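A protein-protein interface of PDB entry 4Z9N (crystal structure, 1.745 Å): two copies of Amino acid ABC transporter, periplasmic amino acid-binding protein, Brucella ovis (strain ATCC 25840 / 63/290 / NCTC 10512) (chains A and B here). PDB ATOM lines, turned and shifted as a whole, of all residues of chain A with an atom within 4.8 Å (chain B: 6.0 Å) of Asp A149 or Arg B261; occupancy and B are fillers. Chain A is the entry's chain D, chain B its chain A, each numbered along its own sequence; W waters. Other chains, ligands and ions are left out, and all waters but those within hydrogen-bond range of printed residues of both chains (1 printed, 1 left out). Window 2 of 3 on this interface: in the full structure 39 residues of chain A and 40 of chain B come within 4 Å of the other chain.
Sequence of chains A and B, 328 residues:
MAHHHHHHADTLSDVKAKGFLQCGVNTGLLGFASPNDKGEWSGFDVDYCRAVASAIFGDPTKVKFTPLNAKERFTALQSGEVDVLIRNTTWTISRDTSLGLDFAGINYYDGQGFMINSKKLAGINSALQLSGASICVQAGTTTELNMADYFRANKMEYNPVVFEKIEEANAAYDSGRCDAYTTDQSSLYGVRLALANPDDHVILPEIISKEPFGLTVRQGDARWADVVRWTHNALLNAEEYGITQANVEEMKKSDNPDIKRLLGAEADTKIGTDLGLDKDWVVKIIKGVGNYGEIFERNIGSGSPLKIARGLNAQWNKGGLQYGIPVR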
ATOM      1  N   LEU A 145      -4.571  18.094  -3.447  1.00  0.00           N
ATOM      2  CA  LEU A 145      -5.374  19.211  -3.946  1.00  0.00           C
ATOM      3  C   LEU A 145      -5.594  19.109  -5.454  1.00  0.00           C
ATOM      4  O   LEU A 145      -6.695  19.369  -5.946  1.00  0.00           O
ATOM      5  CB  LEU A 145      -4.705  20.553  -3.606  1.00  0.00           C
ATOM      6  CG  LEU A 145      -4.354  20.749  -2.120  1.00  0.00           C
ATOM      7  CD1 LEU A 145      -3.657  22.086  -1.869  1.00  0.00           C
ATOM      8  CD2 LEU A 145      -5.612  20.623  -1.258  1.00  0.00           C
ATOM      9  N   ASN A 146      -4.540  18.760  -6.191  1.00  0.00           N
ATOM     10  CA  ASN A 146      -4.657  18.669  -7.650  1.00  0.00           C
ATOM     11  C   ASN A 146      -5.644  17.578  -8.057  1.00  0.00           C
ATOM     12  O   ASN A 146      -6.351  17.736  -9.055  1.00  0.00           O
ATOM     13  CB  ASN A 146      -3.324  18.367  -8.321  1.00  0.00           C
ATOM     14  CG  ASN A 146      -2.293  19.459  -8.122  1.00  0.00           C
ATOM     15  OD1 ASN A 146      -2.620  20.636  -8.019  1.00  0.00           O
ATOM     16  ND2 ASN A 146      -1.027  19.061  -8.066  1.00  0.00           N
ATOM     17  N   MET A 147      -5.661  16.458  -7.327  1.00  0.00           N
ATOM     18  CA  MET A 147      -6.562  15.369  -7.706  1.00  0.00           C
ATOM     19  C   MET A 147      -8.010  15.816  -7.565  1.00  0.00           C
ATOM     20  O   MET A 147      -8.828  15.561  -8.438  1.00  0.00           O
ATOM     21  CB  MET A 147      -6.338  14.115  -6.876  1.00  0.00           C
ATOM     22  CG  MET A 147      -7.369  13.039  -7.197  1.00  0.00           C
ATOM     23  SD  MET A 147      -6.927  11.417  -6.558  1.00  0.00           S
ATOM     24  CE  MET A 147      -6.780  11.751  -4.801  1.00  0.00           C
ATOM     25  N   ALA A 148      -8.324  16.485  -6.466  1.00  0.00           N
ATOM     26  CA  ALA A 148      -9.668  17.010  -6.292  1.00  0.00           C
ATOM     27  C   ALA A 148     -10.024  17.901  -7.489  1.00  0.00           C
ATOM     28  O   ALA A 148     -11.113  17.778  -8.066  1.00  0.00           O
ATOM     29  CB  ALA A 148      -9.782  17.776  -4.979  1.00  0.00           C
ATOM     30  N   ASP A 149      -9.104  18.795  -7.865  1.00  0.00           N
ATOM     31  CA  ASP A 149      -9.343  19.714  -8.984  1.00  0.00           C
ATOM     32  C   ASP A 149      -9.673  18.948 -10.260  1.00  0.00           C
ATOM     33  O   ASP A 149     -10.597  19.299 -11.010  1.00  0.00           O
ATOM     34  CB  ASP A 149      -8.118  20.590  -9.265  1.00  0.00           C
ATOM     35  CG  ASP A 149      -7.872  21.652  -8.212  1.00  0.00           C
ATOM     36  OD1 ASP A 149      -8.778  21.949  -7.405  1.00  0.00           O
ATOM     37  OD2 ASP A 149      -6.747  22.206  -8.221  1.00  0.00           O
ATOM     38  N   TYR A 150      -8.872  17.923 -10.526  1.00  0.00           N
ATOM     39  CA  TYR A 150      -8.970  17.174 -11.777  1.00  0.00           C
ATOM     40  C   TYR A 150     -10.292  16.408 -11.875  1.00  0.00           C
ATOM     41  O   TYR A 150     -10.923  16.361 -12.932  1.00  0.00           O
ATOM     42  CB  TYR A 150      -7.782  16.213 -11.892  1.00  0.00           C
ATOM     43  CG  TYR A 150      -7.709  15.408 -13.170  1.00  0.00           C
ATOM     44  CD1 TYR A 150      -7.393  16.011 -14.379  1.00  0.00           C
ATOM     45  CD2 TYR A 150      -7.919  14.031 -13.154  1.00  0.00           C
ATOM     46  CE1 TYR A 150      -7.310  15.270 -15.555  1.00  0.00           C
ATOM     47  CE2 TYR A 150      -7.827  13.277 -14.322  1.00  0.00           C
ATOM     48  CZ  TYR A 150      -7.521  13.903 -15.516  1.00  0.00           C
ATOM     49  OH  TYR A 150      -7.433  13.160 -16.674  1.00  0.00           O
ATOM     50  N   PHE A 151     -10.726  15.830 -10.760  1.00  0.00           N
ATOM     51  CA  PHE A 151     -11.956  15.055 -10.770  1.00  0.00           C
ATOM     52  C   PHE A 151     -13.168  15.967 -10.854  1.00  0.00           C
ATOM     53  O   PHE A 151     -14.137  15.627 -11.524  1.00  0.00           O
ATOM     54  CB  PHE A 151     -12.027  14.148  -9.533  1.00  0.00           C
ATOM     55  CG  PHE A 151     -11.354  12.832  -9.736  1.00  0.00           C
ATOM     56  CD1 PHE A 151      -9.981  12.766  -9.953  1.00  0.00           C
ATOM     57  CD2 PHE A 151     -12.094  11.661  -9.754  1.00  0.00           C
ATOM     58  CE1 PHE A 151      -9.362  11.548 -10.168  1.00  0.00           C
ATOM     59  CE2 PHE A 151     -11.489  10.447  -9.974  1.00  0.00           C
ATOM     60  CZ  PHE A 151     -10.123  10.383 -10.185  1.00  0.00           C
ATOM     61  N   ARG A 152     -13.099  17.130 -10.198  1.00  0.00           N
ATOM     62  CA  ARG A 152     -14.175  18.117 -10.284  1.00  0.00           C
ATOM     63  C   ARG A 152     -14.326  18.603 -11.723  1.00  0.00           C
ATOM     64  O   ARG A 152     -15.426  18.626 -12.284  1.00  0.00           O
ATOM     65  CB  ARG A 152     -13.911  19.320  -9.370  1.00  0.00           C
ATOM     66  CG  ARG A 152     -14.930  20.436  -9.557  1.00  0.00           C
ATOM     67  CD  ARG A 152     -14.706  21.617  -8.592  1.00  0.00           C
ATOM     68  NE  ARG A 152     -13.273  21.802  -8.369  1.00  0.00           N
ATOM     69  CZ  ARG A 152     -12.664  21.713  -7.186  1.00  0.00           C
ATOM     70  NH1 ARG A 152     -13.368  21.541  -6.082  1.00  0.00           N
ATOM     71  NH2 ARG A 152     -11.346  21.857  -7.094  1.00  0.00           N
ATOM     72  N   ALA A 153     -13.202  18.985 -12.318  1.00  0.00           N
ATOM     73  CA  ALA A 153     -13.203  19.589 -13.644  1.00  0.00           C
ATOM     74  C   ALA A 153     -13.744  18.621 -14.676  1.00  0.00           C
ATOM     75  O   ALA A 153     -14.445  19.011 -15.616  1.00  0.00           O
ATOM     76  CB  ALA A 153     -11.789  20.039 -14.021  1.00  0.00           C
ATOM     77  N   TYR B 241      -2.380  29.088 -19.987  1.00  0.00           N
ATOM     78  CA  TYR B 241      -3.796  28.770 -19.832  1.00  0.00           C
ATOM     79  C   TYR B 241      -4.713  29.503 -20.831  1.00  0.00           C
ATOM     80  O   TYR B 241      -5.940  29.386 -20.755  1.00  0.00           O
ATOM     81  CB  TYR B 241      -4.248  29.091 -18.404  1.00  0.00           C
ATOM     82  CG  TYR B 241      -3.510  28.336 -17.309  1.00  0.00           C
ATOM     83  CD1 TYR B 241      -2.851  27.148 -17.570  1.00  0.00           C
ATOM     84  CD2 TYR B 241      -3.482  28.825 -16.010  1.00  0.00           C
ATOM     85  CE1 TYR B 241      -2.188  26.457 -16.559  1.00  0.00           C
ATOM     86  CE2 TYR B 241      -2.817  28.146 -14.997  1.00  0.00           C
ATOM     87  CZ  TYR B 241      -2.168  26.964 -15.281  1.00  0.00           C
ATOM     88  OH  TYR B 241      -1.513  26.287 -14.273  1.00  0.00           O
ATOM     89  N   ASN B 256     -12.322  25.635 -15.240  1.00  0.00           N
ATOM     90  CA  ASN B 256     -10.990  25.111 -14.954  1.00  0.00           C
ATOM     91  C   ASN B 256     -10.532  25.609 -13.584  1.00  0.00           C
ATOM     92  O   ASN B 256     -10.343  26.805 -13.397  1.00  0.00           O
ATOM     93  CB  ASN B 256     -10.009  25.549 -16.050  1.00  0.00           C
ATOM     94  CG  ASN B 256      -8.638  24.914 -15.920  1.00  0.00           C
ATOM     95  OD1 ASN B 256      -8.138  24.697 -14.823  1.00  0.00           O
ATOM     96  ND2 ASN B 256      -8.009  24.638 -17.058  1.00  0.00           N
ATOM     97  N   PRO B 257     -10.350  24.690 -12.622  1.00  0.00           N
ATOM     98  CA  PRO B 257      -9.932  25.130 -11.283  1.00  0.00           C
ATOM     99  C   PRO B 257      -8.570  25.837 -11.284  1.00  0.00           C
ATOM    100  O   PRO B 257      -8.366  26.755 -10.482  1.00  0.00           O
ATOM    101  CB  PRO B 257      -9.885  23.815 -10.478  1.00  0.00           C
ATOM    102  CG  PRO B 257     -10.806  22.878 -11.228  1.00  0.00           C
ATOM    103  CD  PRO B 257     -10.647  23.243 -12.668  1.00  0.00           C
ATOM    104  N   ASP B 258      -7.658  25.455 -12.176  1.00  0.00           N
ATOM    105  CA  ASP B 258      -6.374  26.164 -12.256  1.00  0.00           C
ATOM    106  C   ASP B 258      -6.555  27.646 -12.558  1.00  0.00           C
ATOM    107  O   ASP B 258      -5.911  28.502 -11.953  1.00  0.00           O
ATOM    108  CB  ASP B 258      -5.478  25.566 -13.330  1.00  0.00           C
ATOM    109  CG  ASP B 258      -5.003  24.184 -12.987  1.00  0.00           C
ATOM    110  OD1 ASP B 258      -5.195  23.747 -11.833  1.00  0.00           O
ATOM    111  OD2 ASP B 258      -4.414  23.547 -13.874  1.00  0.00           O
ATOM    112  N   ILE B 259      -7.418  27.916 -13.530  1.00  0.00           N
ATOM    113  CA  ILE B 259      -7.714  29.269 -13.984  1.00  0.00           C
ATOM    114  C   ILE B 259      -8.473  30.032 -12.894  1.00  0.00           C
ATOM    115  O   ILE B 259      -8.123  31.173 -12.577  1.00  0.00           O
ATOM    116  CB  ILE B 259      -8.490  29.221 -15.315  1.00  0.00           C
ATOM    117  CG1 ILE B 259      -7.582  28.622 -16.391  1.00  0.00           C
ATOM    118  CG2 ILE B 259      -8.986  30.613 -15.697  1.00  0.00           C
ATOM    119  CD1 ILE B 259      -8.233  28.384 -17.714  1.00  0.00           C
ATOM    120  N   LYS B 260      -9.511  29.408 -12.337  1.00  0.00           N
ATOM    121  CA  LYS B 260     -10.246  30.017 -11.230  1.00  0.00           C
ATOM    122  C   LYS B 260      -9.283  30.398 -10.103  1.00  0.00           C
ATOM    123  O   LYS B 260      -9.362  31.511  -9.574  1.00  0.00           O
ATOM    124  CB  LYS B 260     -11.353  29.082 -10.716  1.00  0.00           C
ATOM    125  N   ARG B 261      -8.346  29.509  -9.772  1.00  0.00           N
ATOM    126  CA  ARG B 261      -7.398  29.772  -8.688  1.00  0.00           C
ATOM    127  C   ARG B 261      -6.435  30.913  -9.057  1.00  0.00           C
ATOM    128  O   ARG B 261      -6.158  31.805  -8.241  1.00  0.00           O
ATOM    129  CB  ARG B 261      -6.618  28.494  -8.332  1.00  0.00           C
ATOM    130  CG  ARG B 261      -5.586  28.649  -7.204  1.00  0.00           C
ATOM    131  CD  ARG B 261      -5.038  27.291  -6.702  1.00  0.00           C
ATOM    132  NE  ARG B 261      -4.357  26.538  -7.759  1.00  0.00           N
ATOM    133  CZ  ARG B 261      -4.884  25.494  -8.382  1.00  0.00           C
ATOM    134  NH1 ARG B 261      -6.097  25.066  -8.051  1.00  0.00           N
ATOM    135  NH2 ARG B 261      -4.194  24.869  -9.326  1.00  0.00           N
ATOM    136  N   LEU B 262      -5.927  30.890 -10.284  1.00  0.00           N
ATOM    137  CA  LEU B 262      -5.007  31.926 -10.748  1.00  0.00           C
ATOM    138  C   LEU B 262      -5.630  33.318 -10.669  1.00  0.00           C
ATOM    139  O   LEU B 262      -4.975  34.280 -10.279  1.00  0.00           O
ATOM    140  CB  LEU B 262      -4.579  31.646 -12.190  1.00  0.00           C
ATOM    141  CG  LEU B 262      -3.579  32.623 -12.801  1.00  0.00           C
ATOM    142  CD1 LEU B 262      -2.240  32.488 -12.067  1.00  0.00           C
ATOM    143  CD2 LEU B 262      -3.417  32.367 -14.290  1.00  0.00           C
ATOM    144  N   LEU B 263      -6.901  33.408 -11.045  1.00  0.00           N
ATOM    145  CA  LEU B 263      -7.562  34.695 -11.215  1.00  0.00           C
ATOM    146  C   LEU B 263      -8.315  35.128  -9.957  1.00  0.00           C
ATOM    147  O   LEU B 263      -9.076  36.086  -9.997  1.00  0.00           O
ATOM    148  CB  LEU B 263      -8.513  34.651 -12.424  1.00  0.00           C
ATOM    149  CG  LEU B 263      -7.805  34.393 -13.766  1.00  0.00           C
ATOM    150  CD1 LEU B 263      -8.746  34.530 -14.952  1.00  0.00           C
ATOM    151  CD2 LEU B 263      -6.614  35.333 -13.949  1.00  0.00           C
ATOM    152  N   GLY B 264      -8.096  34.422  -8.850  1.00  0.00           N
ATOM    153  CA  GLY B 264      -8.658  34.816  -7.566  1.00  0.00           C
ATOM    154  C   GLY B 264     -10.151  34.597  -7.421  1.00  0.00           C
ATOM    155  O   GLY B 264     -10.817  35.274  -6.639  1.00  0.00           O
ATOM    156  N   ALA B 265     -10.683  33.640  -8.172  1.00  0.00           N
ATOM    157  CA  ALA B 265     -12.111  33.377  -8.166  1.00  0.00           C
ATOM    158  C   ALA B 265     -12.476  32.224  -7.234  1.00  0.00           C
ATOM    159  O   ALA B 265     -13.649  31.977  -6.997  1.00  0.00           O
ATOM    160  CB  ALA B 265     -12.599  33.087  -9.583  1.00  0.00           C
ATOM    161  N   GLU B 266     -11.479  31.516  -6.708  1.00  0.00           N
ATOM    162  CA  GLU B 266     -11.755  30.410  -5.794  1.00  0.00           C
ATOM    163  C   GLU B 266     -12.214  30.954  -4.448  1.00  0.00           C
ATOM    164  O   GLU B 266     -11.740  31.994  -3.994  1.00  0.00           O
ATOM    165  CB  GLU B 266     -10.526  29.510  -5.618  1.00  0.00           C
ATOM    166  N   THR B 269      -9.763  31.718  -1.174  1.00  0.00           N
ATOM    167  CA  THR B 269      -8.362  31.711  -1.559  1.00  0.00           C
ATOM    168  C   THR B 269      -7.591  32.816  -0.850  1.00  0.00           C
ATOM    169  O   THR B 269      -8.103  33.916  -0.633  1.00  0.00           O
ATOM    170  CB  THR B 269      -8.186  31.864  -3.077  1.00  0.00           C
ATOM    171  OG1 THR B 269      -6.799  31.760  -3.395  1.00  0.00           O
ATOM    172  CG2 THR B 269      -8.719  33.217  -3.558  1.00  0.00           C
ATOM    173  N   ILE B 271      -4.199  33.413  -1.823  1.00  0.00           N
ATOM    174  CA  ILE B 271      -2.946  33.463  -2.580  1.00  0.00           C
ATOM    175  C   ILE B 271      -2.478  34.893  -2.748  1.00  0.00           C
ATOM    176  O   ILE B 271      -1.352  35.228  -2.397  1.00  0.00           O
ATOM    177  CB  ILE B 271      -3.089  32.780  -3.944  1.00  0.00           C
ATOM    178  CG1 ILE B 271      -3.200  31.273  -3.733  1.00  0.00           C
ATOM    179  CG2 ILE B 271      -1.916  33.137  -4.857  1.00  0.00           C
ATOM    180  CD1 ILE B 271      -3.356  30.508  -5.012  1.00  0.00           C
ATOM    181  N   LYS B 279      -6.819  39.894  -3.964  1.00  0.00           N
ATOM    182  CA  LYS B 279      -7.208  38.566  -4.444  1.00  0.00           C
ATOM    183  C   LYS B 279      -7.093  38.449  -5.967  1.00  0.00           C
ATOM    184  O   LYS B 279      -6.631  37.426  -6.493  1.00  0.00           O
ATOM    185  CB  LYS B 279      -8.637  38.283  -3.968  1.00  0.00           C
ATOM    186  CG  LYS B 279      -9.202  36.893  -4.195  1.00  0.00           C
ATOM    187  CD  LYS B 279     -10.752  36.985  -4.082  1.00  0.00           C
ATOM    188  CE  LYS B 279     -11.368  35.982  -3.101  1.00  0.00           C
ATOM    189  NZ  LYS B 279     -11.785  34.663  -3.684  1.00  0.00           N
ATOM    190  N   VAL B 327       0.773  28.409  -9.528  1.00  0.00           N
ATOM    191  CA  VAL B 327       0.074  29.262  -8.578  1.00  0.00           C
ATOM    192  C   VAL B 327      -0.894  28.348  -7.836  1.00  0.00           C
ATOM    193  O   VAL B 327      -2.051  28.184  -8.230  1.00  0.00           O
ATOM    194  CB  VAL B 327      -0.602  30.419  -9.302  1.00  0.00           C
ATOM    195  CG1 VAL B 327      -1.359  31.303  -8.340  1.00  0.00           C
ATOM    196  CG2 VAL B 327       0.489  31.226 -10.017  1.00  0.00           C
ATOM    197  N   ARG B 328      -0.371  27.764  -6.756  1.00  0.00           N
ATOM    198  CA  ARG B 328      -0.925  26.595  -6.066  1.00  0.00           C
ATOM    199  C   ARG B 328      -0.598  26.724  -4.580  1.00  0.00           C
ATOM    200  O   ARG B 328       0.268  27.554  -4.229  1.00  0.00           O
ATOM    201  CB  ARG B 328      -0.321  25.295  -6.651  1.00  0.00           C
ATOM    202  CG  ARG B 328      -0.436  24.017  -5.793  1.00  0.00           C
ATOM    203  CD  ARG B 328      -1.704  23.212  -6.091  1.00  0.00           C
ATOM    204  NE  ARG B 328      -2.886  23.783  -5.450  1.00  0.00           N
ATOM    205  CZ  ARG B 328      -4.136  23.399  -5.694  1.00  0.00           C
ATOM    206  NH1 ARG B 328      -5.140  24.005  -5.063  1.00  0.00           N
ATOM    207  NH2 ARG B 328      -4.390  22.428  -6.566  1.00  0.00           N
ATOM    208  OXT ARG B 328      -1.163  26.015  -3.722  1.00  0.00           O
HETATM  209  O   HOH W   1      -7.783  23.093  -5.039  1.00  0.00           O
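The guanidinium group (NH2) of Arg A152 lies within salt-bridge range of the side-chain carboxylate (OD1) of Asp A149.
The guanidinium group of Arg B261 lies within hydrogen-bond range of the backbone carbonyl oxygen of Val B327 (2.9 Å).
OD1 of Asp B258 lies within salt-bridge range of NH2 of Arg B261, 2.9 Å away.
Among the printed residues, merely in contact across the chains: Leu A145 with Arg B328, Asp A149 with Pro B257, Arg A152 with Pro B257 and Ala A153 with Pro B257.
No position is printed for both chains.
Water W1 bridges the guanidinium group (NH1) of Arg B328 (2.8 Å) and the side-chain carboxylate (OD1) of Asp A149 (2.8 Å).
The guanidinium group of Arg B261 is in salt-bridge range of the side-chain carboxylate of Asp A149.
The guanidinium group of Arg B328 lies within hydrogen-bond range of the side-chain amide oxygen of Asn A146 (2.9 Å).
The side-chain carboxylate of Asp A149 is in salt-bridge range of the guanidinium group of Arg B328.
Printed residues of chain B within 4 Å of Leu A145: Arg B328 (3.5 Å).
Arg B261 touches just one residue of chain A: Asp A149 (2.9 Å).
Printed residues of chain A within 4 Å of Arg B328: Leu A145 (3.5 Å), Asn A146 (2.9 Å) and Asp A149 (2.9 Å).
The nearest residue of chain A that does not touch Arg B261 is Asn A146 (4.7 Å).
Of the 9 printed residues of chain A, 5 touch a printed residue of chain B.
Hydrophobic or aromatic side chains of chain A within 4 Å of the printed part of chain B: Leu A145 and Ala A153.
Printed residues of chain B that touch a printed residue of chain A: Pro B257, Arg B261 and Arg B328.
Among the printed residues, Asp or Glu carboxylates within 4 Å of a Lys or Arg side-chain nitrogen of the other chain: Asp A149 with Arg B261 and Asp A149 with Arg B328.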
